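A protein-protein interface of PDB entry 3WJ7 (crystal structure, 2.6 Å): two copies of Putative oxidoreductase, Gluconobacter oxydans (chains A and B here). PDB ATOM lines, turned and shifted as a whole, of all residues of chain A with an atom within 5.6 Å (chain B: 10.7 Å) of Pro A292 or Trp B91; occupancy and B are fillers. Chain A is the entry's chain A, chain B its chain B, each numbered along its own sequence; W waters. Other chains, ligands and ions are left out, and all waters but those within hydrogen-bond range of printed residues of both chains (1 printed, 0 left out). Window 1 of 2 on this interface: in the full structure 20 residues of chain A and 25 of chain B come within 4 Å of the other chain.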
ATOM      1  N   VAL A 150     -16.000  17.196  27.823  1.00  0.00           N
ATOM      2  CA  VAL A 150     -14.608  17.104  28.253  1.00  0.00           C
ATOM      3  C   VAL A 150     -14.060  18.485  28.606  1.00  0.00           C
ATOM      4  O   VAL A 150     -14.368  19.452  27.944  1.00  0.00           O
ATOM      5  CB  VAL A 150     -13.762  16.368  27.221  1.00  0.00           C
ATOM      6  CG1 VAL A 150     -12.321  16.823  27.288  1.00  0.00           C
ATOM      7  CG2 VAL A 150     -13.899  14.868  27.435  1.00  0.00           C
ATOM      8  N   ILE A 151     -13.288  18.579  29.683  1.00  0.00           N
ATOM      9  CA  ILE A 151     -13.138  19.863  30.343  1.00  0.00           C
ATOM     10  C   ILE A 151     -11.810  20.581  30.082  1.00  0.00           C
ATOM     11  O   ILE A 151     -11.808  21.834  29.873  1.00  0.00           O
ATOM     12  CB  ILE A 151     -13.597  19.795  31.841  1.00  0.00           C
ATOM     13  CG1 ILE A 151     -15.081  20.166  31.926  1.00  0.00           C
ATOM     14  CG2 ILE A 151     -12.808  20.694  32.782  1.00  0.00           C
ATOM     15  CD1 ILE A 151     -15.637  20.990  30.755  1.00  0.00           C
ATOM     16  N   GLY A 152     -10.700  19.827  30.062  1.00  0.00           N
ATOM     17  CA  GLY A 152      -9.408  20.483  29.812  1.00  0.00           C
ATOM     18  C   GLY A 152      -8.685  19.965  28.581  1.00  0.00           C
ATOM     19  O   GLY A 152      -9.124  19.007  27.920  1.00  0.00           O
ATOM     20  N   SER A 281     -15.177  34.386  37.918  1.00  0.00           N
ATOM     21  CA  SER A 281     -14.598  34.046  36.621  1.00  0.00           C
ATOM     22  C   SER A 281     -15.509  34.341  35.411  1.00  0.00           C
ATOM     23  O   SER A 281     -15.071  34.973  34.477  1.00  0.00           O
ATOM     24  CB  SER A 281     -14.152  32.583  36.658  1.00  0.00           C
ATOM     25  OG  SER A 281     -13.878  32.101  35.374  1.00  0.00           O
ATOM     26  N   GLU A 282     -16.768  33.916  35.427  1.00  0.00           N
ATOM     27  CA  GLU A 282     -17.692  34.279  34.347  1.00  0.00           C
ATOM     28  C   GLU A 282     -17.884  35.769  34.275  1.00  0.00           C
ATOM     29  O   GLU A 282     -17.921  36.320  33.173  1.00  0.00           O
ATOM     30  CB  GLU A 282     -19.058  33.636  34.504  1.00  0.00           C
ATOM     31  CG  GLU A 282     -19.058  32.120  34.371  1.00  0.00           C
ATOM     32  CD  GLU A 282     -20.413  31.466  34.684  1.00  0.00           C
ATOM     33  OE1 GLU A 282     -21.488  32.079  34.428  1.00  0.00           O
ATOM     34  OE2 GLU A 282     -20.408  30.303  35.180  1.00  0.00           O
ATOM     35  N   ALA A 285     -14.488  37.545  32.810  1.00  0.00           N
ATOM     36  CA  ALA A 285     -14.467  37.360  31.357  1.00  0.00           C
ATOM     37  C   ALA A 285     -15.526  38.174  30.624  1.00  0.00           C
ATOM     38  O   ALA A 285     -15.189  38.824  29.618  1.00  0.00           O
ATOM     39  CB  ALA A 285     -14.572  35.921  30.978  1.00  0.00           C
ATOM     40  N   ILE A 290     -13.782  38.574  27.046  1.00  0.00           N
ATOM     41  CA  ILE A 290     -12.994  37.405  26.659  1.00  0.00           C
ATOM     42  C   ILE A 290     -13.745  36.118  27.002  1.00  0.00           C
ATOM     43  O   ILE A 290     -14.874  36.181  27.476  1.00  0.00           O
ATOM     44  CB  ILE A 290     -11.576  37.396  27.275  1.00  0.00           C
ATOM     45  CG1 ILE A 290     -11.652  37.354  28.799  1.00  0.00           C
ATOM     46  CG2 ILE A 290     -10.779  38.583  26.763  1.00  0.00           C
ATOM     47  CD1 ILE A 290     -10.356  37.016  29.480  1.00  0.00           C
ATOM     48  N   GLU A 291     -13.134  34.966  26.728  1.00  0.00           N
ATOM     49  CA  GLU A 291     -13.738  33.675  27.057  1.00  0.00           C
ATOM     50  C   GLU A 291     -13.257  33.279  28.411  1.00  0.00           C
ATOM     51  O   GLU A 291     -12.065  33.352  28.696  1.00  0.00           O
ATOM     52  CB  GLU A 291     -13.377  32.580  26.047  1.00  0.00           C
ATOM     53  CG  GLU A 291     -14.354  32.497  24.873  1.00  0.00           C
ATOM     54  CD  GLU A 291     -14.284  31.171  24.111  1.00  0.00           C
ATOM     55  OE1 GLU A 291     -14.460  30.093  24.748  1.00  0.00           O
ATOM     56  OE2 GLU A 291     -14.075  31.212  22.868  1.00  0.00           O
ATOM     57  N   PRO A 292     -14.187  32.874  29.273  1.00  0.00           N
ATOM     58  CA  PRO A 292     -13.745  32.398  30.590  1.00  0.00           C
ATOM     59  C   PRO A 292     -13.094  31.041  30.442  1.00  0.00           C
ATOM     60  O   PRO A 292     -13.514  30.273  29.609  1.00  0.00           O
ATOM     61  CB  PRO A 292     -15.034  32.304  31.397  1.00  0.00           C
ATOM     62  CG  PRO A 292     -16.139  32.315  30.381  1.00  0.00           C
ATOM     63  CD  PRO A 292     -15.647  32.964  29.126  1.00  0.00           C
ATOM     64  N   ARG A 293     -12.051  30.760  31.202  1.00  0.00           N
ATOM     65  CA  ARG A 293     -11.447  29.437  31.149  1.00  0.00           C
ATOM     66  C   ARG A 293     -12.274  28.466  31.967  1.00  0.00           C
ATOM     67  O   ARG A 293     -12.226  27.250  31.733  1.00  0.00           O
ATOM     68  CB  ARG A 293     -10.035  29.462  31.723  1.00  0.00           C
ATOM     69  CG  ARG A 293      -9.030  30.250  30.898  1.00  0.00           C
ATOM     70  CD  ARG A 293      -7.630  30.026  31.443  1.00  0.00           C
ATOM     71  NE  ARG A 293      -7.153  28.687  31.101  1.00  0.00           N
ATOM     72  CZ  ARG A 293      -6.318  27.972  31.844  1.00  0.00           C
ATOM     73  NH1 ARG A 293      -5.852  28.460  32.992  1.00  0.00           N
ATOM     74  NH2 ARG A 293      -5.968  26.759  31.442  1.00  0.00           N
ATOM     75  N   VAL A 294     -13.021  29.026  32.923  1.00  0.00           N
ATOM     76  CA  VAL A 294     -13.746  28.284  33.927  1.00  0.00           C
ATOM     77  C   VAL A 294     -15.120  28.909  34.107  1.00  0.00           C
ATOM     78  O   VAL A 294     -15.236  30.118  34.122  1.00  0.00           O
ATOM     79  CB  VAL A 294     -12.941  28.345  35.204  1.00  0.00           C
ATOM     80  CG1 VAL A 294     -13.805  28.237  36.437  1.00  0.00           C
ATOM     81  CG2 VAL A 294     -11.901  27.251  35.178  1.00  0.00           C
ATOM     82  N   THR A 295     -16.168  28.083  34.195  1.00  0.00           N
ATOM     83  CA  THR A 295     -17.564  28.543  34.386  1.00  0.00           C
ATOM     84  C   THR A 295     -18.237  27.602  35.398  1.00  0.00           C
ATOM     85  O   THR A 295     -17.690  26.534  35.678  1.00  0.00           O
ATOM     86  CB  THR A 295     -18.387  28.466  33.061  1.00  0.00           C
ATOM     87  OG1 THR A 295     -18.681  27.114  32.768  1.00  0.00           O
ATOM     88  CG2 THR A 295     -17.639  28.989  31.848  1.00  0.00           C
ATOM     89  N   GLU A 297     -20.653  25.746  34.463  1.00  0.00           N
ATOM     90  CA  GLU A 297     -20.762  24.556  33.594  1.00  0.00           C
ATOM     91  C   GLU A 297     -19.469  23.726  33.640  1.00  0.00           C
ATOM     92  O   GLU A 297     -19.482  22.509  33.521  1.00  0.00           O
ATOM     93  CB  GLU A 297     -21.135  24.955  32.130  1.00  0.00           C
ATOM     94  CG  GLU A 297     -21.654  23.807  31.242  1.00  0.00           C
ATOM     95  CD  GLU A 297     -21.392  23.967  29.723  1.00  0.00           C
ATOM     96  OE1 GLU A 297     -20.249  23.706  29.239  1.00  0.00           O
ATOM     97  OE2 GLU A 297     -22.351  24.322  28.990  1.00  0.00           O
ATOM     98  N   THR A 298     -18.345  24.395  33.829  1.00  0.00           N
ATOM     99  CA  THR A 298     -17.072  23.701  33.973  1.00  0.00           C
ATOM    100  C   THR A 298     -16.964  22.960  35.296  1.00  0.00           C
ATOM    101  O   THR A 298     -16.666  21.766  35.326  1.00  0.00           O
ATOM    102  CB  THR A 298     -15.879  24.646  33.699  1.00  0.00           C
ATOM    103  OG1 THR A 298     -15.498  24.405  32.350  1.00  0.00           O
ATOM    104  CG2 THR A 298     -14.634  24.340  34.554  1.00  0.00           C
ATOM    105  N   ASP B  87     -22.351  26.345  16.242  1.00  0.00           N
ATOM    106  CA  ASP B  87     -22.632  26.818  17.595  1.00  0.00           C
ATOM    107  C   ASP B  87     -22.808  28.347  17.652  1.00  0.00           C
ATOM    108  O   ASP B  87     -22.470  29.080  16.714  1.00  0.00           O
ATOM    109  CB  ASP B  87     -21.479  26.422  18.536  1.00  0.00           C
ATOM    110  CG  ASP B  87     -21.471  24.936  18.878  1.00  0.00           C
ATOM    111  OD1 ASP B  87     -22.530  24.398  19.292  1.00  0.00           O
ATOM    112  OD2 ASP B  87     -20.393  24.314  18.752  1.00  0.00           O
ATOM    113  N   TYR B  88     -23.339  28.817  18.775  1.00  0.00           N
ATOM    114  CA  TYR B  88     -23.328  30.236  19.085  1.00  0.00           C
ATOM    115  C   TYR B  88     -22.597  30.459  20.424  1.00  0.00           C
ATOM    116  O   TYR B  88     -23.093  30.045  21.480  1.00  0.00           O
ATOM    117  CB  TYR B  88     -24.758  30.833  19.096  1.00  0.00           C
ATOM    118  CG  TYR B  88     -24.730  32.322  19.372  1.00  0.00           C
ATOM    119  CD1 TYR B  88     -24.598  33.261  18.326  1.00  0.00           C
ATOM    120  CD2 TYR B  88     -24.765  32.793  20.686  1.00  0.00           C
ATOM    121  CE1 TYR B  88     -24.524  34.621  18.593  1.00  0.00           C
ATOM    122  CE2 TYR B  88     -24.692  34.148  20.966  1.00  0.00           C
ATOM    123  CZ  TYR B  88     -24.570  35.060  19.926  1.00  0.00           C
ATOM    124  OH  TYR B  88     -24.499  36.396  20.264  1.00  0.00           O
ATOM    125  N   ARG B  89     -21.422  31.097  20.371  1.00  0.00           N
ATOM    126  CA  ARG B  89     -20.619  31.428  21.578  1.00  0.00           C
ATOM    127  C   ARG B  89     -20.358  30.266  22.603  1.00  0.00           C
ATOM    128  O   ARG B  89     -20.145  30.503  23.798  1.00  0.00           O
ATOM    129  CB  ARG B  89     -21.156  32.713  22.276  1.00  0.00           C
ATOM    130  CG  ARG B  89     -20.551  34.037  21.788  1.00  0.00           C
ATOM    131  CD  ARG B  89     -21.179  35.288  22.428  1.00  0.00           C
ATOM    132  NE  ARG B  89     -20.962  36.497  21.610  1.00  0.00           N
ATOM    133  CZ  ARG B  89     -21.602  37.670  21.731  1.00  0.00           C
ATOM    134  NH1 ARG B  89     -22.537  37.862  22.659  1.00  0.00           N
ATOM    135  NH2 ARG B  89     -21.298  38.671  20.904  1.00  0.00           N
ATOM    136  N   LEU B  90     -20.329  29.025  22.117  1.00  0.00           N
ATOM    137  CA  LEU B  90     -19.994  27.829  22.926  1.00  0.00           C
ATOM    138  C   LEU B  90     -18.574  27.828  23.591  1.00  0.00           C
ATOM    139  O   LEU B  90     -17.570  27.753  22.890  1.00  0.00           O
ATOM    140  CB  LEU B  90     -20.104  26.610  22.020  1.00  0.00           C
ATOM    141  CG  LEU B  90     -19.777  25.244  22.608  1.00  0.00           C
ATOM    142  CD1 LEU B  90     -21.080  24.564  23.034  1.00  0.00           C
ATOM    143  CD2 LEU B  90     -18.992  24.408  21.597  1.00  0.00           C
ATOM    144  N   TRP B  91     -18.477  27.895  24.918  1.00  0.00           N
ATOM    145  CA  TRP B  91     -17.174  27.766  25.572  1.00  0.00           C
ATOM    146  C   TRP B  91     -16.488  26.426  25.179  1.00  0.00           C
ATOM    147  O   TRP B  91     -17.190  25.401  25.074  1.00  0.00           O
ATOM    148  CB  TRP B  91     -17.345  27.861  27.089  1.00  0.00           C
ATOM    149  CG  TRP B  91     -16.124  27.477  27.796  1.00  0.00           C
ATOM    150  CD1 TRP B  91     -15.180  28.312  28.259  1.00  0.00           C
ATOM    151  CD2 TRP B  91     -15.667  26.137  28.079  1.00  0.00           C
ATOM    152  NE1 TRP B  91     -14.154  27.596  28.827  1.00  0.00           N
ATOM    153  CE2 TRP B  91     -14.421  26.257  28.723  1.00  0.00           C
ATOM    154  CE3 TRP B  91     -16.191  24.845  27.838  1.00  0.00           C
ATOM    155  CZ2 TRP B  91     -13.677  25.145  29.138  1.00  0.00           C
ATOM    156  CZ3 TRP B  91     -15.459  23.738  28.241  1.00  0.00           C
ATOM    157  CH2 TRP B  91     -14.210  23.896  28.890  1.00  0.00           C
ATOM    158  N   VAL B  92     -15.151  26.414  24.978  1.00  0.00           N
ATOM    159  CA  VAL B  92     -14.405  25.161  24.651  1.00  0.00           C
ATOM    160  C   VAL B  92     -13.070  25.146  25.368  1.00  0.00           C
ATOM    161  O   VAL B  92     -12.532  26.179  25.681  1.00  0.00           O
ATOM    162  CB  VAL B  92     -14.097  25.002  23.122  1.00  0.00           C
ATOM    163  CG1 VAL B  92     -15.261  24.374  22.353  1.00  0.00           C
ATOM    164  CG2 VAL B  92     -13.686  26.337  22.502  1.00  0.00           C
ATOM    165  N   PRO B  93     -12.467  23.980  25.568  1.00  0.00           N
ATOM    166  CA  PRO B  93     -11.148  24.213  26.186  1.00  0.00           C
ATOM    167  C   PRO B  93     -10.051  24.533  25.163  1.00  0.00           C
ATOM    168  O   PRO B  93      -8.906  24.802  25.523  1.00  0.00           O
ATOM    169  CB  PRO B  93     -10.852  22.896  26.893  1.00  0.00           C
ATOM    170  CG  PRO B  93     -11.724  21.861  26.230  1.00  0.00           C
ATOM    171  CD  PRO B  93     -12.809  22.547  25.439  1.00  0.00           C
ATOM    172  N   ASP B  94     -10.382  24.485  23.884  1.00  0.00           N
ATOM    173  CA  ASP B  94      -9.391  24.788  22.846  1.00  0.00           C
ATOM    174  C   ASP B  94      -9.918  25.908  21.910  1.00  0.00           C
ATOM    175  O   ASP B  94     -10.238  25.638  20.761  1.00  0.00           O
ATOM    176  CB  ASP B  94      -9.063  23.524  22.036  1.00  0.00           C
ATOM    177  CG  ASP B  94     -10.309  22.865  21.483  1.00  0.00           C
ATOM    178  OD1 ASP B  94     -11.425  23.072  22.033  1.00  0.00           O
ATOM    179  OD2 ASP B  94     -10.200  22.155  20.487  1.00  0.00           O
ATOM    180  N   PRO B  95     -10.004  27.149  22.404  1.00  0.00           N
ATOM    181  CA  PRO B  95     -10.570  28.279  21.598  1.00  0.00           C
ATOM    182  C   PRO B  95      -9.791  28.516  20.308  1.00  0.00           C
ATOM    183  O   PRO B  95     -10.407  28.741  19.270  1.00  0.00           O
ATOM    184  CB  PRO B  95     -10.419  29.514  22.522  1.00  0.00           C
ATOM    185  CG  PRO B  95     -10.114  28.954  23.899  1.00  0.00           C
ATOM    186  CD  PRO B  95      -9.443  27.612  23.696  1.00  0.00           C
ATOM    187  N   GLU B  96      -8.463  28.443  20.352  1.00  0.00           N
ATOM    188  CA  GLU B  96      -7.663  28.658  19.139  1.00  0.00           C
ATOM    189  C   GLU B  96      -7.792  27.580  18.093  1.00  0.00           C
ATOM    190  O   GLU B  96      -7.812  27.888  16.888  1.00  0.00           O
ATOM    191  CB  GLU B  96      -6.184  28.878  19.461  1.00  0.00           C
ATOM    192  CG  GLU B  96      -5.886  30.089  20.329  1.00  0.00           C
ATOM    193  CD  GLU B  96      -4.423  30.519  20.203  1.00  0.00           C
ATOM    194  OE1 GLU B  96      -3.964  30.647  19.030  1.00  0.00           O
ATOM    195  OE2 GLU B  96      -3.726  30.738  21.248  1.00  0.00           O
ATOM    196  N   MET B  98     -10.513  25.796  17.737  1.00  0.00           N
ATOM    197  CA  MET B  98     -11.856  25.977  17.175  1.00  0.00           C
ATOM    198  C   MET B  98     -11.873  27.153  16.205  1.00  0.00           C
ATOM    199  O   MET B  98     -12.449  27.042  15.130  1.00  0.00           O
ATOM    200  CB  MET B  98     -12.969  26.095  18.228  1.00  0.00           C
ATOM    201  CG  MET B  98     -13.480  24.743  18.754  1.00  0.00           C
ATOM    202  SD  MET B  98     -13.968  23.357  17.645  1.00  0.00           S
ATOM    203  CE  MET B  98     -12.448  22.418  17.352  1.00  0.00           C
ATOM    204  N   MET B  99     -11.220  28.252  16.558  1.00  0.00           N
ATOM    205  CA  MET B  99     -11.020  29.312  15.594  1.00  0.00           C
ATOM    206  C   MET B  99     -10.425  28.860  14.231  1.00  0.00           C
ATOM    207  O   MET B  99     -10.918  29.289  13.158  1.00  0.00           O
ATOM    208  CB  MET B  99     -10.145  30.406  16.148  1.00  0.00           C
ATOM    209  CG  MET B  99      -9.928  31.480  15.087  1.00  0.00           C
ATOM    210  SD  MET B  99      -9.040  32.927  15.668  1.00  0.00           S
ATOM    211  CE  MET B  99      -7.476  32.082  15.977  1.00  0.00           C
ATOM    212  N   ILE B 151     -10.745  41.977  20.450  1.00  0.00           N
ATOM    213  CA  ILE B 151     -10.022  41.525  21.620  1.00  0.00           C
ATOM    214  C   ILE B 151     -10.116  40.051  22.109  1.00  0.00           C
ATOM    215  O   ILE B 151      -9.172  39.581  22.749  1.00  0.00           O
ATOM    216  CB  ILE B 151      -9.962  42.599  22.761  1.00  0.00           C
ATOM    217  CG1 ILE B 151     -11.346  43.055  23.177  1.00  0.00           C
ATOM    218  CG2 ILE B 151      -9.092  43.792  22.337  1.00  0.00           C
ATOM    219  CD1 ILE B 151     -11.916  42.197  24.270  1.00  0.00           C
ATOM    220  N   GLY B 152     -11.183  39.316  21.809  1.00  0.00           N
ATOM    221  CA  GLY B 152     -11.217  37.890  22.237  1.00  0.00           C
ATOM    222  C   GLY B 152     -11.133  36.950  21.046  1.00  0.00           C
ATOM    223  O   GLY B 152     -11.430  37.358  19.932  1.00  0.00           O
ATOM    224  N   ILE B 153     -10.734  35.700  21.270  1.00  0.00           N
ATOM    225  CA  ILE B 153     -10.762  34.651  20.244  1.00  0.00           C
ATOM    226  C   ILE B 153     -12.125  34.563  19.542  1.00  0.00           C
ATOM    227  O   ILE B 153     -12.181  34.539  18.295  1.00  0.00           O
ATOM    228  CB  ILE B 153     -10.376  33.227  20.769  1.00  0.00           C
ATOM    229  CG1 ILE B 153      -9.528  33.270  22.047  1.00  0.00           C
ATOM    230  CG2 ILE B 153      -9.664  32.420  19.690  1.00  0.00           C
ATOM    231  CD1 ILE B 153      -8.206  32.488  22.012  1.00  0.00           C
ATOM    232  N   TYR B 154     -13.219  34.539  20.314  1.00  0.00           N
ATOM    233  CA  TYR B 154     -14.578  34.521  19.712  1.00  0.00           C
ATOM    234  C   TYR B 154     -14.795  35.656  18.716  1.00  0.00           C
ATOM    235  O   TYR B 154     -15.179  35.387  17.612  1.00  0.00           O
ATOM    236  CB  TYR B 154     -15.758  34.477  20.716  1.00  0.00           C
ATOM    237  CG  TYR B 154     -17.115  34.571  19.952  1.00  0.00           C
ATOM    238  CD1 TYR B 154     -17.664  33.445  19.263  1.00  0.00           C
ATOM    239  CD2 TYR B 154     -17.816  35.796  19.868  1.00  0.00           C
ATOM    240  CE1 TYR B 154     -18.859  33.546  18.545  1.00  0.00           C
ATOM    241  CE2 TYR B 154     -19.015  35.901  19.164  1.00  0.00           C
ATOM    242  CZ  TYR B 154     -19.539  34.793  18.493  1.00  0.00           C
ATOM    243  OH  TYR B 154     -20.742  34.951  17.789  1.00  0.00           O
ATOM    244  N   LYS B 191     -29.638  24.626  24.885  1.00  0.00           N
ATOM    245  CA  LYS B 191     -28.391  24.521  25.655  1.00  0.00           C
ATOM    246  C   LYS B 191     -28.468  24.901  27.154  1.00  0.00           C
ATOM    247  O   LYS B 191     -28.220  24.047  27.998  1.00  0.00           O
ATOM    248  CB  LYS B 191     -27.235  25.276  24.958  1.00  0.00           C
ATOM    249  CG  LYS B 191     -26.144  24.389  24.386  1.00  0.00           C
ATOM    250  CD  LYS B 191     -25.845  24.754  22.931  1.00  0.00           C
ATOM    251  CE  LYS B 191     -25.326  23.563  22.111  1.00  0.00           C
ATOM    252  NZ  LYS B 191     -25.307  23.809  20.633  1.00  0.00           N
ATOM    253  N   PRO B 192     -28.772  26.171  27.505  1.00  0.00           N
ATOM    254  CA  PRO B 192     -29.102  27.331  26.707  1.00  0.00           C
ATOM    255  C   PRO B 192     -27.810  28.080  26.377  1.00  0.00           C
ATOM    256  O   PRO B 192     -26.789  27.919  27.051  1.00  0.00           O
ATOM    257  CB  PRO B 192     -29.924  28.167  27.679  1.00  0.00           C
ATOM    258  CG  PRO B 192     -29.381  27.817  29.038  1.00  0.00           C
ATOM    259  CD  PRO B 192     -28.502  26.595  28.892  1.00  0.00           C
ATOM    260  N   THR B 193     -27.848  28.767  25.261  1.00  0.00           N
ATOM    261  CA  THR B 193     -27.123  30.014  24.970  1.00  0.00           C
ATOM    262  C   THR B 193     -26.640  30.772  26.219  1.00  0.00           C
ATOM    263  O   THR B 193     -27.322  30.776  27.235  1.00  0.00           O
ATOM    264  CB  THR B 193     -28.149  30.841  24.129  1.00  0.00           C
ATOM    265  OG1 THR B 193     -27.728  30.886  22.775  1.00  0.00           O
ATOM    266  CG2 THR B 193     -28.466  32.214  24.653  1.00  0.00           C
ATOM    267  N   PRO B 194     -25.458  31.399  26.180  1.00  0.00           N
ATOM    268  CA  PRO B 194     -25.069  32.174  27.392  1.00  0.00           C
ATOM    269  C   PRO B 194     -26.046  33.277  27.797  1.00  0.00           C
ATOM    270  O   PRO B 194     -26.285  33.451  28.991  1.00  0.00           O
ATOM    271  CB  PRO B 194     -23.706  32.751  27.027  1.00  0.00           C
ATOM    272  CG  PRO B 194     -23.181  31.779  26.029  1.00  0.00           C
ATOM    273  CD  PRO B 194     -24.364  31.397  25.190  1.00  0.00           C
ATOM    274  N   THR B 195     -26.646  33.979  26.841  1.00  0.00           N
ATOM    275  CA  THR B 195     -27.668  34.945  27.191  1.00  0.00           C
ATOM    276  C   THR B 195     -28.941  34.333  27.800  1.00  0.00           C
ATOM    277  O   THR B 195     -29.493  34.897  28.751  1.00  0.00           O
ATOM    278  CB  THR B 195     -27.960  35.895  26.043  1.00  0.00           C
ATOM    279  OG1 THR B 195     -26.718  36.470  25.618  1.00  0.00           O
ATOM    280  CG2 THR B 195     -28.912  37.022  26.488  1.00  0.00           C
ATOM    281  N   ARG B 293      -3.777  37.617  29.747  1.00  0.00           N
ATOM    282  CA  ARG B 293      -4.935  37.425  28.906  1.00  0.00           C
ATOM    283  C   ARG B 293      -5.718  38.731  28.766  1.00  0.00           C
ATOM    284  O   ARG B 293      -6.500  38.925  27.848  1.00  0.00           O
ATOM    285  CB  ARG B 293      -5.811  36.335  29.485  1.00  0.00           C
ATOM    286  CG  ARG B 293      -5.453  34.943  28.987  1.00  0.00           C
ATOM    287  CD  ARG B 293      -6.563  33.941  29.319  1.00  0.00           C
ATOM    288  NE  ARG B 293      -6.156  32.577  28.956  1.00  0.00           N
ATOM    289  CZ  ARG B 293      -5.477  31.741  29.746  1.00  0.00           C
ATOM    290  NH1 ARG B 293      -5.125  32.094  30.990  1.00  0.00           N
ATOM    291  NH2 ARG B 293      -5.161  30.536  29.292  1.00  0.00           N
ATOM    292  N   VAL B 294      -5.468  39.643  29.680  1.00  0.00           N
ATOM    293  CA  VAL B 294      -6.303  40.796  29.857  1.00  0.00           C
ATOM    294  C   VAL B 294      -5.353  41.918  30.135  1.00  0.00           C
ATOM    295  O   VAL B 294      -4.441  41.740  30.947  1.00  0.00           O
ATOM    296  CB  VAL B 294      -7.236  40.586  31.070  1.00  0.00           C
ATOM    297  CG1 VAL B 294      -7.399  41.840  31.865  1.00  0.00           C
ATOM    298  CG2 VAL B 294      -8.573  40.011  30.625  1.00  0.00           C
HETATM  299  O   HOH W   1     -10.659  35.012  24.645  1.00  0.00           O
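The guanidinium group (NH2) of Arg B293 sits close to the guanidinium group (NE) of Arg A293 (3.3 Å).
O of Pro A292 sits at hydrogen-bond distance from NE1 of Trp B91, 2.9 Å away.
Printed residues of chain B within 4 Å of Val A150: Pro B93.
No residue of chain B comes within 4 Å of Ala A285.
Pro A292 touches one residue of chain B.
No residue of chain B comes within 4 Å of Val A294.
Glu A297 touches none of the printed residues of chain B.
Of chain A, only Ile A151, Glu A291, Pro A292, Arg A293 and Thr A298 come within 4 Å of Trp B91.
Pro B194 touches none of the printed residues of chain A.
Printed residues of chain A within 4 Å of Arg B293: Arg A293.
The nearest residue of chain B that does not touch Pro A292 is Val B92 (5.8 Å).
Arg A293 touches its own counterpart, Arg B293.
Positions printed for both chains: 151, 152, 293 and 294.
Of the 10 pairs that touch across the chains among the printed residues, 1 has its exchanged pair printed and touching as well.
The backbone carbonyl oxygen (O) of Ala A285 is in hydrogen-bond range of the backbone NH (N) of Ile A290 (2.9 Å).
The side-chain hydroxyl (OG1) of Thr A295 is in hydrogen-bond range of the backbone NH (N) of Thr A298 (2.9 Å).
Among the printed residues, merely in contact across the chains: Val A150 with Pro B93 (3.97 Å), Ile A151 with Trp B91 (3.3 Å), Ile A151 with Pro B93 (3.3 Å), Ile A290 with Val B294 (3.7 Å), Glu A291 with Trp B91 (3.7 Å), Glu A291 with Val B92 (3.8 Å), Arg A293 with Trp B91 (3.5 Å) and Thr A298 with Trp B91 (3.7 Å).
Water W1 bridges N of Glu A291 (3.2 Å) and N of Ile B153 (3.4 Å).
Hydrophobic or aromatic side chains of chain B within 4 Å of the printed part of chain A: Trp B91, Pro B93 and Val B294.
Along chain B the printed residues that touch a printed residue of chain A span positions 91 to 294.
Hydrophobic or aromatic side chains of chain A that line the printed part of chain B: Ile A151 and Ile A290.
Among the printed residues, 10 pairs touch across the chains.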
